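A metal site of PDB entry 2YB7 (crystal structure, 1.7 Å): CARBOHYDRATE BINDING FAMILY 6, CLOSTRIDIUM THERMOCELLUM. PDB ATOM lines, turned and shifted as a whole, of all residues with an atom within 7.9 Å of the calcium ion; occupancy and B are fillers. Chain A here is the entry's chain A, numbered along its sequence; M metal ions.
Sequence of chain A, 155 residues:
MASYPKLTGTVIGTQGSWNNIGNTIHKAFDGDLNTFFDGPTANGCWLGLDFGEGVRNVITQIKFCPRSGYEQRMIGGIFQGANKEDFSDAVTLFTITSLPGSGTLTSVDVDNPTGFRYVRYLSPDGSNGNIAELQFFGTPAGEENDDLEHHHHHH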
ATOM      1  N   THR A  24      14.741   4.274   5.539  1.00  0.00           N
ATOM      2  CA  THR A  24      15.928   3.646   4.904  1.00  0.00           C
ATOM      3  C   THR A  24      15.709   2.125   4.765  1.00  0.00           C
ATOM      4  O   THR A  24      14.636   1.564   5.252  1.00  0.00           O
ATOM      5  CB  THR A  24      17.154   3.833   5.736  1.00  0.00           C
ATOM      6  OG1 THR A  24      16.913   3.160   6.989  1.00  0.00           O
ATOM      7  CG2 THR A  24      17.441   5.315   6.015  1.00  0.00           C
ATOM      8  N   ILE A  25      16.686   1.440   4.162  1.00  0.00           N
ATOM      9  CA  ILE A  25      16.572  -0.007   4.027  1.00  0.00           C
ATOM     10  C   ILE A  25      16.356  -0.720   5.346  1.00  0.00           C
ATOM     11  O   ILE A  25      15.839  -1.800   5.358  1.00  0.00           O
ATOM     12  CB  ILE A  25      17.802  -0.618   3.295  1.00  0.00           C
ATOM     13  CG1 ILE A  25      19.108  -0.184   4.035  1.00  0.00           C
ATOM     14  CG2 ILE A  25      17.697  -0.096   1.749  1.00  0.00           C
ATOM     15  CD1 ILE A  25      20.425  -0.723   3.215  1.00  0.00           C
ATOM     16  N   HIS A  26      16.857  -0.151   6.469  1.00  0.00           N
ATOM     17  CA  HIS A  26      16.793  -0.860   7.704  1.00  0.00           C
ATOM     18  C   HIS A  26      15.299  -1.042   8.117  1.00  0.00           C
ATOM     19  O   HIS A  26      15.069  -1.886   8.949  1.00  0.00           O
ATOM     20  CB  HIS A  26      17.472   0.060   8.746  1.00  0.00           C
ATOM     21  CG  HIS A  26      18.969  -0.013   8.579  1.00  0.00           C
ATOM     22  ND1 HIS A  26      19.712   0.862   7.783  1.00  0.00           N
ATOM     23  CD2 HIS A  26      19.787  -1.044   8.922  1.00  0.00           C
ATOM     24  CE1 HIS A  26      20.955   0.400   7.708  1.00  0.00           C
ATOM     25  NE2 HIS A  26      21.032  -0.734   8.422  1.00  0.00           N
ATOM     26  N   LYS A  27      14.358  -0.225   7.601  1.00  0.00           N
ATOM     27  CA  LYS A  27      12.941  -0.447   7.998  1.00  0.00           C
ATOM     28  C   LYS A  27      12.417  -1.759   7.440  1.00  0.00           C
ATOM     29  O   LYS A  27      11.354  -2.219   7.848  1.00  0.00           O
ATOM     30  CB  LYS A  27      12.090   0.644   7.382  1.00  0.00           C
ATOM     31  CG  LYS A  27      12.485   2.086   7.795  1.00  0.00           C
ATOM     32  CD  LYS A  27      12.541   2.254   9.333  1.00  0.00           C
ATOM     33  CE  LYS A  27      12.788   3.764   9.658  1.00  0.00           C
ATOM     34  NZ  LYS A  27      13.447   3.785  11.006  1.00  0.00           N
ATOM     35  N   ALA A  28      13.121  -2.437   6.524  1.00  0.00           N
ATOM     36  CA  ALA A  28      12.607  -3.696   6.044  1.00  0.00           C
ATOM     37  C   ALA A  28      13.019  -4.868   6.912  1.00  0.00           C
ATOM     38  O   ALA A  28      12.672  -6.023   6.645  1.00  0.00           O
ATOM     39  CB  ALA A  28      13.132  -3.943   4.563  1.00  0.00           C
ATOM     40  N   PHE A  29      13.747  -4.612   8.033  1.00  0.00           N
ATOM     41  CA  PHE A  29      14.245  -5.699   8.876  1.00  0.00           C
ATOM     42  C   PHE A  29      13.896  -5.456  10.325  1.00  0.00           C
ATOM     43  O   PHE A  29      14.488  -6.128  11.179  1.00  0.00           O
ATOM     44  CB  PHE A  29      15.795  -5.834   8.734  1.00  0.00           C
ATOM     45  CG  PHE A  29      16.196  -6.061   7.331  1.00  0.00           C
ATOM     46  CD1 PHE A  29      16.307  -7.374   6.739  1.00  0.00           C
ATOM     47  CD2 PHE A  29      16.501  -4.910   6.547  1.00  0.00           C
ATOM     48  CE1 PHE A  29      16.715  -7.493   5.391  1.00  0.00           C
ATOM     49  CE2 PHE A  29      16.909  -5.042   5.192  1.00  0.00           C
ATOM     50  CZ  PHE A  29      17.029  -6.314   4.642  1.00  0.00           C
ATOM     51  N   ASP A  30      12.988  -4.574  10.595  1.00  0.00           N
ATOM     52  CA  ASP A  30      12.758  -4.164  11.969  1.00  0.00           C
ATOM     53  C   ASP A  30      11.562  -4.891  12.616  1.00  0.00           C
ATOM     54  O   ASP A  30      11.298  -4.651  13.821  1.00  0.00           O
ATOM     55  CB  ASP A  30      12.457  -2.677  12.108  1.00  0.00           C
ATOM     56  CG  ASP A  30      11.283  -2.223  11.301  1.00  0.00           C
ATOM     57  OD1 ASP A  30      10.576  -3.007  10.603  1.00  0.00           O
ATOM     58  OD2 ASP A  30      11.093  -0.990  11.274  1.00  0.00           O
ATOM     59  N   GLY A  31      10.997  -5.817  11.907  1.00  0.00           N
ATOM     60  CA  GLY A  31       9.841  -6.637  12.521  1.00  0.00           C
ATOM     61  C   GLY A  31       8.533  -5.934  12.461  1.00  0.00           C
ATOM     62  O   GLY A  31       7.503  -6.532  12.930  1.00  0.00           O
ATOM     63  N   ASP A  32       8.446  -4.752  11.937  1.00  0.00           N
ATOM     64  CA  ASP A  32       7.152  -4.006  11.940  1.00  0.00           C
ATOM     65  C   ASP A  32       6.632  -3.918  10.513  1.00  0.00           C
ATOM     66  O   ASP A  32       7.337  -3.356   9.615  1.00  0.00           O
ATOM     67  CB  ASP A  32       7.444  -2.581  12.376  1.00  0.00           C
ATOM     68  CG  ASP A  32       6.184  -1.817  12.642  1.00  0.00           C
ATOM     69  OD1 ASP A  32       5.081  -2.246  12.240  1.00  0.00           O
ATOM     70  OD2 ASP A  32       6.228  -0.719  13.205  1.00  0.00           O
ATOM     71  N   LEU A  33       5.500  -4.536  10.204  1.00  0.00           N
ATOM     72  CA  LEU A  33       4.994  -4.482   8.849  1.00  0.00           C
ATOM     73  C   LEU A  33       4.466  -3.129   8.509  1.00  0.00           C
ATOM     74  O   LEU A  33       4.132  -2.914   7.338  1.00  0.00           O
ATOM     75  CB  LEU A  33       3.879  -5.531   8.677  1.00  0.00           C
ATOM     76  CG  LEU A  33       4.272  -6.964   9.188  1.00  0.00           C
ATOM     77  CD1 LEU A  33       3.086  -7.885   8.691  1.00  0.00           C
ATOM     78  CD2 LEU A  33       5.546  -7.441   8.470  1.00  0.00           C
ATOM     79  N   ASN A  34       4.353  -2.200   9.491  1.00  0.00           N
ATOM     80  CA  ASN A  34       3.879  -0.843   9.161  1.00  0.00           C
ATOM     81  C   ASN A  34       5.035   0.053   8.743  1.00  0.00           C
ATOM     82  O   ASN A  34       4.757   1.154   8.259  1.00  0.00           O
ATOM     83  CB  ASN A  34       3.273  -0.189  10.417  1.00  0.00           C
ATOM     84  CG  ASN A  34       2.089  -1.005  10.917  1.00  0.00           C
ATOM     85  OD1 ASN A  34       1.139  -1.119  10.170  1.00  0.00           O
ATOM     86  ND2 ASN A  34       2.254  -1.731  12.003  1.00  0.00           N
ATOM     87  N   THR A  35       6.272  -0.376   8.957  1.00  0.00           N
ATOM     88  CA  THR A  35       7.356   0.507   8.521  1.00  0.00           C
ATOM     89  C   THR A  35       7.931  -0.019   7.247  1.00  0.00           C
ATOM     90  O   THR A  35       8.014  -1.269   7.070  1.00  0.00           O
ATOM     91  CB  THR A  35       8.470   0.489   9.507  1.00  0.00           C
ATOM     92  OG1 THR A  35       8.999  -0.824   9.733  1.00  0.00           O
ATOM     93  CG2 THR A  35       8.047   1.050  10.888  1.00  0.00           C
ATOM     94  N   PHE A  36       8.511   0.820   6.421  1.00  0.00           N
ATOM     95  CA  PHE A  36       8.868   0.328   5.063  1.00  0.00           C
ATOM     96  C   PHE A  36      10.118   1.101   4.610  1.00  0.00           C
ATOM     97  O   PHE A  36      10.363   2.204   5.064  1.00  0.00           O
ATOM     98  CB  PHE A  36       7.722   0.606   4.014  1.00  0.00           C
ATOM     99  CG  PHE A  36       7.139   1.997   4.109  1.00  0.00           C
ATOM    100  CD1 PHE A  36       6.078   2.264   5.006  1.00  0.00           C
ATOM    101  CD2 PHE A  36       7.716   3.047   3.315  1.00  0.00           C
ATOM    102  CE1 PHE A  36       5.594   3.582   5.123  1.00  0.00           C
ATOM    103  CE2 PHE A  36       7.274   4.387   3.454  1.00  0.00           C
ATOM    104  CZ  PHE A  36       6.182   4.639   4.343  1.00  0.00           C
ATOM    105  N   PHE A  37      10.786   0.535   3.618  1.00  0.00           N
ATOM    106  CA  PHE A  37      11.875   1.228   2.910  1.00  0.00           C
ATOM    107  C   PHE A  37      11.218   2.011   1.773  1.00  0.00           C
ATOM    108  O   PHE A  37      10.401   1.491   0.964  1.00  0.00           O
ATOM    109  CB  PHE A  37      12.769   0.101   2.324  1.00  0.00           C
ATOM    110  CG  PHE A  37      13.794   0.649   1.339  1.00  0.00           C
ATOM    111  CD1 PHE A  37      14.449   1.833   1.616  1.00  0.00           C
ATOM    112  CD2 PHE A  37      14.021  -0.044   0.147  1.00  0.00           C
ATOM    113  CE1 PHE A  37      15.460   2.367   0.729  1.00  0.00           C
ATOM    114  CE2 PHE A  37      15.066   0.472  -0.787  1.00  0.00           C
ATOM    115  CZ  PHE A  37      15.783   1.676  -0.500  1.00  0.00           C
ATOM    116  N   CYS A  65       6.784  -8.524   2.931  1.00  0.00           N
ATOM    117  CA  CYS A  65       5.453  -7.870   3.018  1.00  0.00           C
ATOM    118  C   CYS A  65       5.634  -6.534   2.252  1.00  0.00           C
ATOM    119  O   CYS A  65       6.640  -5.827   2.460  1.00  0.00           O
ATOM    120  CB  CYS A  65       5.301  -7.537   4.555  1.00  0.00           C
ATOM    121  SG  CYS A  65       3.742  -6.553   4.814  1.00  0.00           S
ATOM    122  N   ILE A 131       9.044  -1.763   0.119  1.00  0.00           N
ATOM    123  CA  ILE A 131       8.837  -3.030   0.726  1.00  0.00           C
ATOM    124  C   ILE A 131       8.827  -2.786   2.202  1.00  0.00           C
ATOM    125  O   ILE A 131       9.581  -1.933   2.696  1.00  0.00           O
ATOM    126  CB  ILE A 131       9.992  -4.051   0.374  1.00  0.00           C
ATOM    127  CG1 ILE A 131       9.793  -5.448   0.991  1.00  0.00           C
ATOM    128  CG2 ILE A 131      11.437  -3.466   0.743  1.00  0.00           C
ATOM    129  CD1 ILE A 131      10.857  -6.464   0.505  1.00  0.00           C
ATOM    130  N   ALA A 132       7.946  -3.487   2.922  1.00  0.00           N
ATOM    131  CA  ALA A 132       7.863  -3.236   4.372  1.00  0.00           C
ATOM    132  C   ALA A 132       8.702  -4.146   5.161  1.00  0.00           C
ATOM    133  O   ALA A 132       9.174  -3.804   6.272  1.00  0.00           O
ATOM    134  CB  ALA A 132       6.324  -3.368   4.881  1.00  0.00           C
ATOM    135  N   GLU A 133       8.885  -5.382   4.720  1.00  0.00           N
ATOM    136  CA  GLU A 133       9.638  -6.286   5.603  1.00  0.00           C
ATOM    137  C   GLU A 133      10.198  -7.392   4.693  1.00  0.00           C
ATOM    138  O   GLU A 133       9.514  -7.831   3.741  1.00  0.00           O
ATOM    139  CB  GLU A 133       8.647  -6.957   6.685  1.00  0.00           C
ATOM    140  CG  GLU A 133       9.481  -7.495   7.856  1.00  0.00           C
ATOM    141  CD  GLU A 133      10.151  -6.352   8.737  1.00  0.00           C
ATOM    142  OE1 GLU A 133       9.676  -5.149   8.693  1.00  0.00           O
ATOM    143  OE2 GLU A 133      11.059  -6.773   9.470  1.00  0.00           O
ATOM    144  N   LEU A 134      11.345  -7.925   5.067  1.00  0.00           N
ATOM    145  CA  LEU A 134      12.017  -8.888   4.140  1.00  0.00           C
ATOM    146  C   LEU A 134      12.747  -9.833   5.086  1.00  0.00           C
ATOM    147  O   LEU A 134      13.485  -9.403   6.013  1.00  0.00           O
ATOM    148  CB  LEU A 134      13.094  -8.108   3.280  1.00  0.00           C
ATOM    149  CG  LEU A 134      14.010  -9.067   2.480  1.00  0.00           C
ATOM    150  CD1 LEU A 134      13.151  -9.838   1.518  1.00  0.00           C
ATOM    151  CD2 LEU A 134      14.992  -8.039   1.696  1.00  0.00           C
HETATM  152 CA    CA M   1       9.286  -2.940   8.501  1.00  0.00          CA
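The side-chain carboxylate of Asp 32 lies within hydrogen-bond range of the backbone NH of Asn 34, at 2.8 Å.
The backbone NH of Gly 31 lies within hydrogen-bond range of the side-chain carboxylate of Glu 133.
N of Ala 132 is in hydrogen-bond range of O of Cys 65 (2.7 Å).
The backbone carbonyl oxygen (O) of Glu 133 lies within hydrogen-bond range of the backbone NH (N) of Cys 65 (2.9 Å).
Six residues have an atom within 4 Å of the calcium ion: Lys 27, Asp 30, Asp 32, Thr 35, Ala 132 and Glu 133.
The nearest printed residue that does not touch the calcium ion is Ala 28 (4.2 Å).
OE1 of Glu 133 binds the calcium ion (2.3 Å).
The backbone carbonyl oxygen (O) of Asp 32 binds the calcium ion, at 2.3 Å.
The calcium ion is bound by the backbone carbonyl oxygen (O) of Lys 27 (2.3 Å).
The calcium ion is bound by the backbone carbonyl oxygen (O) of Ala 132 (2.4 Å).
OG1 of Thr 35 binds the calcium ion.
OD1 of Asp 30 binds the calcium ion, at 2.5 Å.
The calcium ion is bound by O of Thr 35, 2.5 Å away.
The calcium ion has seven donor atoms within binding distance.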
